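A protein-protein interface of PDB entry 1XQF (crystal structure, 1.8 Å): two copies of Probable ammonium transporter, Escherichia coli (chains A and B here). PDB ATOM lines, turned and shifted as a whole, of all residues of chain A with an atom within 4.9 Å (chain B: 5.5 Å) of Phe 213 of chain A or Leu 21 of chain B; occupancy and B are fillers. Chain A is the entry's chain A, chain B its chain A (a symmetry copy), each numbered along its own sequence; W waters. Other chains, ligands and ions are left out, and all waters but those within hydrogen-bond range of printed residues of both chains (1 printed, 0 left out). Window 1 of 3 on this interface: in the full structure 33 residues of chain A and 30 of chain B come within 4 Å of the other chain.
SG of Cys 56 of chain B sits at hydrogen-bond distance from O of Phe 52 of chain B.
The side-chain sulfur (SG) of Cys 56 of chain B lies within hydrogen-bond range of the side-chain sulfur (SG) of Cys 109 of chain B (3.8 Å).
Tyr 209 of chain A touches Leu 21 of chain B.
CZ of Phe 52 of chain B touches OH of Tyr 209 of chain A, at 3.4 Å.
CD1 of Ile 210 of chain A touches O of Ala 18 of chain B, 3.8 Å away.
CD1 of Ile 210 of chain A touches C of Leu 21 of chain B (3.8 Å).
Phe 22 of chain B touches Ile 210 of chain A.
O of Ile 25 of chain B touches CG1 of Ile 210 of chain A, at 3.6 Å.
Phe 213 of chain A touches Leu 21 of chain B.
Phe 231 of chain A touches Thr 17 of chain B.
Phe 231 of chain A touches Ala 18 of chain B (CZ to N, 3.9 Å).
CG1 of Val 235 of chain A touches SG of Cys 56 of chain B, at 3.7 Å.
Of chain B, only Leu 21 (3.7 Å) comes within 4 Å of Phe 213 of chain A.
Of the printed residues of chain B, Val 235 of chain A touches Cys 56 (3.7 Å).
Printed residues of chain A within 4 Å of Thr 17 of chain B: Phe 231.
Leu 19 of chain B touches none of the printed residues of chain A.
Leu 21 of chain B touches just these residues of chain A: Tyr 209 (3.96 Å), Ile 210 (3.8 Å) and Phe 213 (3.7 Å).
Printed residues of chain A within 4 Å of Phe 22 of chain B: Ile 210.
Of the printed residues of chain A, Ile 25 of chain B touches Ile 210.
The nearest residue of chain A that does not touch Leu 21 of chain B is Val 235 of chain A (4.4 Å).
Of the 14 printed residues of chain A, 5 touch a printed residue of chain B.
Hydrophobic or aromatic side chains of chain A that line the printed part of chain B: Tyr 209, Ile 210, Phe 213, Phe 231 and Val 235.
Of the 15 printed residues of chain B, 7 touch a printed residue of chain A.
Hydrophobic or aromatic side chains of chain B within 4 Å of the printed part of chain A: Leu 21, Phe 22 and Phe 52.
Among the printed residues, 10 pairs touch across the chains.
Among the printed residues, no Asp or Glu carboxylate lies within 4 Å of a Lys or Arg side-chain nitrogen of the other chain.
Position printed for both chains: 16.
Of the 10 pairs that touch across the chains among the printed residues, none has its exchanged pair printed and touching as well.
Water W1 lies within hydrogen-bond range of O of Val 235 of chain A (2.8 Å), OH of Tyr 209 of chain A (2.8 Å) and SG of Cys 56 of chain B (3.6 Å).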
ATOM      1  N   CYS A  16       8.093 -11.068  21.152  1.00  0.00           N
ATOM      2  CA  CYS A  16       7.044 -10.088  20.768  1.00  0.00           C
ATOM      3  C   CYS A  16       7.464  -9.297  19.516  1.00  0.00           C
ATOM      4  O   CYS A  16       6.621  -8.978  18.654  1.00  0.00           O
ATOM      5  CB  CYS A  16       6.715  -9.117  21.925  1.00  0.00           C
ATOM      6  SG  CYS A  16       5.733  -9.819  23.313  1.00  0.00           S
ATOM      7  N   TYR A 209      -4.003 -10.867  13.622  1.00  0.00           N
ATOM      8  CA  TYR A 209      -4.540 -11.150  14.972  1.00  0.00           C
ATOM      9  C   TYR A 209      -3.494 -11.773  15.930  1.00  0.00           C
ATOM     10  O   TYR A 209      -3.276 -11.262  17.058  1.00  0.00           O
ATOM     11  CB  TYR A 209      -5.783 -12.054  14.848  1.00  0.00           C
ATOM     12  CG  TYR A 209      -6.363 -12.585  16.163  1.00  0.00           C
ATOM     13  CD1 TYR A 209      -6.956 -11.720  17.090  1.00  0.00           C
ATOM     14  CD2 TYR A 209      -6.333 -13.957  16.461  1.00  0.00           C
ATOM     15  CE1 TYR A 209      -7.507 -12.202  18.303  1.00  0.00           C
ATOM     16  CE2 TYR A 209      -6.877 -14.449  17.667  1.00  0.00           C
ATOM     17  CZ  TYR A 209      -7.460 -13.567  18.581  1.00  0.00           C
ATOM     18  OH  TYR A 209      -8.001 -14.047  19.769  1.00  0.00           O
ATOM     19  N   ILE A 210      -2.877 -12.871  15.495  1.00  0.00           N
ATOM     20  CA  ILE A 210      -1.836 -13.565  16.286  1.00  0.00           C
ATOM     21  C   ILE A 210      -0.619 -12.645  16.581  1.00  0.00           C
ATOM     22  O   ILE A 210      -0.184 -12.522  17.736  1.00  0.00           O
ATOM     23  CB  ILE A 210      -1.417 -14.927  15.629  1.00  0.00           C
ATOM     24  CG1 ILE A 210      -2.625 -15.905  15.509  1.00  0.00           C
ATOM     25  CG2 ILE A 210      -0.262 -15.615  16.422  1.00  0.00           C
ATOM     26  CD1 ILE A 210      -3.359 -16.222  16.840  1.00  0.00           C
ATOM     27  N   GLY A 211      -0.093 -11.976  15.556  1.00  0.00           N
ATOM     28  CA  GLY A 211       0.983 -10.995  15.769  1.00  0.00           C
ATOM     29  C   GLY A 211       0.633  -9.839  16.713  1.00  0.00           C
ATOM     30  O   GLY A 211       1.510  -9.330  17.430  1.00  0.00           O
ATOM     31  N   TRP A 212      -0.645  -9.437  16.726  1.00  0.00           N
ATOM     32  CA  TRP A 212      -1.148  -8.320  17.559  1.00  0.00           C
ATOM     33  C   TRP A 212      -1.005  -8.573  19.070  1.00  0.00           C
ATOM     34  O   TRP A 212      -1.052  -7.626  19.860  1.00  0.00           O
ATOM     35  CB  TRP A 212      -2.617  -7.987  17.218  1.00  0.00           C
ATOM     36  CG  TRP A 212      -2.983  -6.490  17.199  1.00  0.00           C
ATOM     37  CD1 TRP A 212      -2.898  -5.592  18.249  1.00  0.00           C
ATOM     38  CD2 TRP A 212      -3.533  -5.749  16.086  1.00  0.00           C
ATOM     39  NE1 TRP A 212      -3.339  -4.337  17.841  1.00  0.00           N
ATOM     40  CE2 TRP A 212      -3.734  -4.408  16.526  1.00  0.00           C
ATOM     41  CE3 TRP A 212      -3.866  -6.088  14.760  1.00  0.00           C
ATOM     42  CZ2 TRP A 212      -4.266  -3.408  15.681  1.00  0.00           C
ATOM     43  CZ3 TRP A 212      -4.390  -5.093  13.915  1.00  0.00           C
ATOM     44  CH2 TRP A 212      -4.580  -3.765  14.387  1.00  0.00           C
ATOM     45  N   PHE A 213      -0.829  -9.830  19.482  1.00  0.00           N
ATOM     46  CA  PHE A 213      -0.514 -10.102  20.907  1.00  0.00           C
ATOM     47  C   PHE A 213       0.902  -9.593  21.293  1.00  0.00           C
ATOM     48  O   PHE A 213       1.118  -9.050  22.401  1.00  0.00           O
ATOM     49  CB  PHE A 213      -0.778 -11.582  21.290  1.00  0.00           C
ATOM     50  CG  PHE A 213      -2.254 -11.958  21.253  1.00  0.00           C
ATOM     51  CD1 PHE A 213      -3.094 -11.615  22.313  1.00  0.00           C
ATOM     52  CD2 PHE A 213      -2.796 -12.620  20.150  1.00  0.00           C
ATOM     53  CE1 PHE A 213      -4.460 -11.934  22.288  1.00  0.00           C
ATOM     54  CE2 PHE A 213      -4.175 -12.936  20.104  1.00  0.00           C
ATOM     55  CZ  PHE A 213      -5.001 -12.594  21.182  1.00  0.00           C
ATOM     56  N   GLY A 214       1.848  -9.726  20.363  1.00  0.00           N
ATOM     57  CA  GLY A 214       3.184  -9.149  20.536  1.00  0.00           C
ATOM     58  C   GLY A 214       3.121  -7.622  20.578  1.00  0.00           C
ATOM     59  O   GLY A 214       3.823  -6.980  21.377  1.00  0.00           O
ATOM     60  N   PHE A 215       2.290  -7.054  19.692  1.00  0.00           N
ATOM     61  CA  PHE A 215       2.079  -5.591  19.542  1.00  0.00           C
ATOM     62  C   PHE A 215       1.498  -4.976  20.840  1.00  0.00           C
ATOM     63  O   PHE A 215       2.057  -4.016  21.396  1.00  0.00           O
ATOM     64  CB  PHE A 215       1.166  -5.379  18.293  1.00  0.00           C
ATOM     65  CG  PHE A 215       0.959  -3.940  17.846  1.00  0.00           C
ATOM     66  CD1 PHE A 215      -0.073  -3.160  18.391  1.00  0.00           C
ATOM     67  CD2 PHE A 215       1.703  -3.409  16.783  1.00  0.00           C
ATOM     68  CE1 PHE A 215      -0.299  -1.841  17.946  1.00  0.00           C
ATOM     69  CE2 PHE A 215       1.478  -2.084  16.322  1.00  0.00           C
ATOM     70  CZ  PHE A 215       0.473  -1.310  16.909  1.00  0.00           C
ATOM     71  N   ASN A 216       0.396  -5.548  21.331  1.00  0.00           N
ATOM     72  CA  ASN A 216      -0.302  -5.030  22.520  1.00  0.00           C
ATOM     73  C   ASN A 216       0.363  -5.429  23.864  1.00  0.00           C
ATOM     74  O   ASN A 216       0.641  -4.569  24.701  1.00  0.00           O
ATOM     75  CB  ASN A 216      -1.784  -5.448  22.512  1.00  0.00           C
ATOM     76  CG  ASN A 216      -2.665  -4.566  21.595  1.00  0.00           C
ATOM     77  OD1 ASN A 216      -2.214  -3.580  20.993  1.00  0.00           O
ATOM     78  ND2 ASN A 216      -3.941  -4.928  21.507  1.00  0.00           N
ATOM     79  N   ALA A 217       0.616  -6.721  24.074  1.00  0.00           N
ATOM     80  CA  ALA A 217       1.214  -7.178  25.341  1.00  0.00           C
ATOM     81  C   ALA A 217       2.677  -6.728  25.495  1.00  0.00           C
ATOM     82  O   ALA A 217       3.089  -6.303  26.587  1.00  0.00           O
ATOM     83  CB  ALA A 217       1.065  -8.688  25.512  1.00  0.00           C
ATOM     84  N   GLY A 218       3.435  -6.780  24.396  1.00  0.00           N
ATOM     85  CA  GLY A 218       4.825  -6.290  24.378  1.00  0.00           C
ATOM     86  C   GLY A 218       4.985  -4.818  24.740  1.00  0.00           C
ATOM     87  O   GLY A 218       6.052  -4.396  25.208  1.00  0.00           O
ATOM     88  N   PHE A 231      -3.121  -8.679  27.333  1.00  0.00           N
ATOM     89  CA  PHE A 231      -3.371  -9.928  26.591  1.00  0.00           C
ATOM     90  C   PHE A 231      -4.862 -10.318  26.634  1.00  0.00           C
ATOM     91  O   PHE A 231      -5.490 -10.516  25.584  1.00  0.00           O
ATOM     92  CB  PHE A 231      -2.472 -11.071  27.123  1.00  0.00           C
ATOM     93  CG  PHE A 231      -2.338 -12.252  26.172  1.00  0.00           C
ATOM     94  CD1 PHE A 231      -3.428 -13.089  25.923  1.00  0.00           C
ATOM     95  CD2 PHE A 231      -1.127 -12.517  25.536  1.00  0.00           C
ATOM     96  CE1 PHE A 231      -3.326 -14.170  25.042  1.00  0.00           C
ATOM     97  CE2 PHE A 231      -1.003 -13.600  24.646  1.00  0.00           C
ATOM     98  CZ  PHE A 231      -2.116 -14.432  24.406  1.00  0.00           C
ATOM     99  N   THR A 234      -7.198  -7.958  24.800  1.00  0.00           N
ATOM    100  CA  THR A 234      -7.092  -8.126  23.330  1.00  0.00           C
ATOM    101  C   THR A 234      -8.036  -9.240  22.843  1.00  0.00           C
ATOM    102  O   THR A 234      -8.788  -9.052  21.877  1.00  0.00           O
ATOM    103  CB  THR A 234      -5.618  -8.357  22.871  1.00  0.00           C
ATOM    104  OG1 THR A 234      -4.832  -7.205  23.208  1.00  0.00           O
ATOM    105  CG2 THR A 234      -5.507  -8.609  21.337  1.00  0.00           C
ATOM    106  N   VAL A 235      -8.013 -10.382  23.529  1.00  0.00           N
ATOM    107  CA  VAL A 235      -8.942 -11.481  23.245  1.00  0.00           C
ATOM    108  C   VAL A 235     -10.406 -11.011  23.311  1.00  0.00           C
ATOM    109  O   VAL A 235     -11.185 -11.267  22.381  1.00  0.00           O
ATOM    110  CB  VAL A 235      -8.749 -12.686  24.218  1.00  0.00           C
ATOM    111  CG1 VAL A 235      -9.759 -13.806  23.909  1.00  0.00           C
ATOM    112  CG2 VAL A 235      -7.316 -13.227  24.154  1.00  0.00           C
ATOM    113  N   CYS B  16       2.747 -19.399  24.731  1.00  0.00           N
ATOM    114  CA  CYS B  16       2.046 -20.685  24.480  1.00  0.00           C
ATOM    115  C   CYS B  16       0.552 -20.449  24.193  1.00  0.00           C
ATOM    116  O   CYS B  16      -0.049 -21.144  23.350  1.00  0.00           O
ATOM    117  CB  CYS B  16       2.213 -21.669  25.660  1.00  0.00           C
ATOM    118  SG  CYS B  16       3.866 -22.456  25.829  1.00  0.00           S
ATOM    119  N   THR B  17      -0.052 -19.492  24.902  1.00  0.00           N
ATOM    120  CA  THR B  17      -1.458 -19.117  24.658  1.00  0.00           C
ATOM    121  C   THR B  17      -1.654 -18.594  23.217  1.00  0.00           C
ATOM    122  O   THR B  17      -2.625 -18.977  22.543  1.00  0.00           O
ATOM    123  CB  THR B  17      -1.992 -18.058  25.672  1.00  0.00           C
ATOM    124  OG1 THR B  17      -1.869 -18.542  27.020  1.00  0.00           O
ATOM    125  CG2 THR B  17      -3.482 -17.719  25.404  1.00  0.00           C
ATOM    126  N   ALA B  18      -0.756 -17.718  22.755  1.00  0.00           N
ATOM    127  CA  ALA B  18      -0.803 -17.220  21.372  1.00  0.00           C
ATOM    128  C   ALA B  18      -0.695 -18.368  20.357  1.00  0.00           C
ATOM    129  O   ALA B  18      -1.422 -18.377  19.365  1.00  0.00           O
ATOM    130  CB  ALA B  18       0.283 -16.150  21.101  1.00  0.00           C
ATOM    131  N   LEU B  19       0.207 -19.320  20.613  1.00  0.00           N
ATOM    132  CA  LEU B  19       0.327 -20.525  19.767  1.00  0.00           C
ATOM    133  C   LEU B  19      -0.957 -21.381  19.735  1.00  0.00           C
ATOM    134  O   LEU B  19      -1.316 -21.910  18.677  1.00  0.00           O
ATOM    135  CB  LEU B  19       1.539 -21.373  20.189  1.00  0.00           C
ATOM    136  CG  LEU B  19       2.952 -20.861  19.835  1.00  0.00           C
ATOM    137  CD1 LEU B  19       4.035 -21.630  20.612  1.00  0.00           C
ATOM    138  CD2 LEU B  19       3.239 -20.919  18.323  1.00  0.00           C
ATOM    139  N   VAL B  20      -1.652 -21.541  20.869  1.00  0.00           N
ATOM    140  CA  VAL B  20      -2.919 -22.310  20.839  1.00  0.00           C
ATOM    141  C   VAL B  20      -4.037 -21.558  20.085  1.00  0.00           C
ATOM    142  O   VAL B  20      -4.848 -22.173  19.380  1.00  0.00           O
ATOM    143  CB  VAL B  20      -3.396 -22.730  22.255  1.00  0.00           C
ATOM    144  CG1 VAL B  20      -4.691 -23.567  22.171  1.00  0.00           C
ATOM    145  CG2 VAL B  20      -2.289 -23.531  22.979  1.00  0.00           C
ATOM    146  N   LEU B  21      -4.107 -20.237  20.241  1.00  0.00           N
ATOM    147  CA  LEU B  21      -5.080 -19.457  19.452  1.00  0.00           C
ATOM    148  C   LEU B  21      -4.844 -19.585  17.914  1.00  0.00           C
ATOM    149  O   LEU B  21      -5.803 -19.653  17.133  1.00  0.00           O
ATOM    150  CB  LEU B  21      -5.101 -17.980  19.896  1.00  0.00           C
ATOM    151  CG  LEU B  21      -5.612 -17.705  21.324  1.00  0.00           C
ATOM    152  CD1 LEU B  21      -5.339 -16.251  21.703  1.00  0.00           C
ATOM    153  CD2 LEU B  21      -7.115 -18.026  21.511  1.00  0.00           C
ATOM    154  N   PHE B  22      -3.566 -19.639  17.520  1.00  0.00           N
ATOM    155  CA  PHE B  22      -3.075 -19.868  16.124  1.00  0.00           C
ATOM    156  C   PHE B  22      -3.607 -21.214  15.558  1.00  0.00           C
ATOM    157  O   PHE B  22      -3.939 -21.304  14.371  1.00  0.00           O
ATOM    158  CB  PHE B  22      -1.527 -19.835  16.164  1.00  0.00           C
ATOM    159  CG  PHE B  22      -0.795 -19.729  14.805  1.00  0.00           C
ATOM    160  CD1 PHE B  22      -1.268 -18.951  13.740  1.00  0.00           C
ATOM    161  CD2 PHE B  22       0.452 -20.365  14.662  1.00  0.00           C
ATOM    162  CE1 PHE B  22      -0.535 -18.852  12.531  1.00  0.00           C
ATOM    163  CE2 PHE B  22       1.202 -20.278  13.467  1.00  0.00           C
ATOM    164  CZ  PHE B  22       0.718 -19.520  12.407  1.00  0.00           C
ATOM    165  N   MET B  23      -3.708 -22.241  16.407  1.00  0.00           N
ATOM    166  CA  MET B  23      -4.336 -23.532  16.000  1.00  0.00           C
ATOM    167  C   MET B  23      -5.775 -23.397  15.432  1.00  0.00           C
ATOM    168  O   MET B  23      -6.151 -24.142  14.516  1.00  0.00           O
ATOM    169  CB  MET B  23      -4.335 -24.564  17.154  1.00  0.00           C
ATOM    170  CG  MET B  23      -2.960 -24.975  17.687  1.00  0.00           C
ATOM    171  SD  MET B  23      -3.056 -26.046  19.171  1.00  0.00           S
ATOM    172  CE  MET B  23      -3.562 -27.590  18.418  1.00  0.00           C
ATOM    173  N   THR B  24      -6.586 -22.484  15.983  1.00  0.00           N
ATOM    174  CA  THR B  24      -7.955 -22.261  15.480  1.00  0.00           C
ATOM    175  C   THR B  24      -7.967 -21.221  14.345  1.00  0.00           C
ATOM    176  O   THR B  24      -8.571 -21.434  13.282  1.00  0.00           O
ATOM    177  CB  THR B  24      -8.931 -21.778  16.607  1.00  0.00           C
ATOM    178  OG1 THR B  24      -8.922 -22.700  17.708  1.00  0.00           O
ATOM    179  CG2 THR B  24     -10.378 -21.639  16.085  1.00  0.00           C
ATOM    180  N   ILE B  25      -7.303 -20.091  14.604  1.00  0.00           N
ATOM    181  CA  ILE B  25      -7.260 -18.931  13.700  1.00  0.00           C
ATOM    182  C   ILE B  25      -5.803 -18.737  13.198  1.00  0.00           C
ATOM    183  O   ILE B  25      -4.988 -18.088  13.874  1.00  0.00           O
ATOM    184  CB  ILE B  25      -7.817 -17.640  14.430  1.00  0.00           C
ATOM    185  CG1 ILE B  25      -9.217 -17.883  15.059  1.00  0.00           C
ATOM    186  CG2 ILE B  25      -7.828 -16.387  13.527  1.00  0.00           C
ATOM    187  CD1 ILE B  25     -10.384 -18.117  14.049  1.00  0.00           C
ATOM    188  N   PRO B  26      -5.468 -19.280  12.001  1.00  0.00           N
ATOM    189  CA  PRO B  26      -6.305 -19.965  10.991  1.00  0.00           C
ATOM    190  C   PRO B  26      -6.141 -21.497  10.803  1.00  0.00           C
ATOM    191  O   PRO B  26      -6.703 -22.044   9.840  1.00  0.00           O
ATOM    192  CB  PRO B  26      -5.820 -19.293   9.697  1.00  0.00           C
ATOM    193  CG  PRO B  26      -4.278 -19.120   9.967  1.00  0.00           C
ATOM    194  CD  PRO B  26      -4.088 -19.120  11.492  1.00  0.00           C
ATOM    195  N   PHE B  52     -15.944 -18.845  17.240  1.00  0.00           N
ATOM    196  CA  PHE B  52     -14.714 -18.530  18.001  1.00  0.00           C
ATOM    197  C   PHE B  52     -14.929 -17.301  18.896  1.00  0.00           C
ATOM    198  O   PHE B  52     -14.646 -17.342  20.098  1.00  0.00           O
ATOM    199  CB  PHE B  52     -13.527 -18.337  17.042  1.00  0.00           C
ATOM    200  CG  PHE B  52     -12.277 -17.757  17.684  1.00  0.00           C
ATOM    201  CD1 PHE B  52     -11.373 -18.577  18.366  1.00  0.00           C
ATOM    202  CD2 PHE B  52     -11.982 -16.389  17.555  1.00  0.00           C
ATOM    203  CE1 PHE B  52     -10.203 -18.045  18.941  1.00  0.00           C
ATOM    204  CE2 PHE B  52     -10.822 -15.849  18.130  1.00  0.00           C
ATOM    205  CZ  PHE B  52      -9.934 -16.676  18.820  1.00  0.00           C
ATOM    206  N   CYS B  56     -15.021 -17.115  23.152  1.00  0.00           N
ATOM    207  CA  CYS B  56     -14.200 -16.137  23.893  1.00  0.00           C
ATOM    208  C   CYS B  56     -15.032 -15.321  24.906  1.00  0.00           C
ATOM    209  O   CYS B  56     -14.596 -15.125  26.046  1.00  0.00           O
ATOM    210  CB  CYS B  56     -13.446 -15.197  22.938  1.00  0.00           C
ATOM    211  SG  CYS B  56     -12.113 -15.938  21.927  1.00  0.00           S
ATOM    212  N   SER B 106      -8.273 -20.609  25.451  1.00  0.00           N
ATOM    213  CA  SER B 106      -7.787 -21.031  24.128  1.00  0.00           C
ATOM    214  C   SER B 106      -8.039 -22.531  23.838  1.00  0.00           C
ATOM    215  O   SER B 106      -8.284 -22.905  22.686  1.00  0.00           O
ATOM    216  CB  SER B 106      -6.317 -20.607  23.893  1.00  0.00           C
ATOM    217  OG  SER B 106      -5.380 -21.390  24.620  1.00  0.00           O
ATOM    218  N   CYS B 109     -11.699 -22.871  22.784  1.00  0.00           N
ATOM    219  CA  CYS B 109     -11.798 -22.418  21.380  1.00  0.00           C
ATOM    220  C   CYS B 109     -11.426 -23.493  20.345  1.00  0.00           C
ATOM    221  O   CYS B 109     -12.149 -23.681  19.363  1.00  0.00           O
ATOM    222  CB  CYS B 109     -10.952 -21.162  21.149  1.00  0.00           C
ATOM    223  SG  CYS B 109     -11.603 -19.656  21.901  1.00  0.00           S
HETATM  224  O   HOH W   1     -10.602 -13.113  20.372  1.00  0.00           O
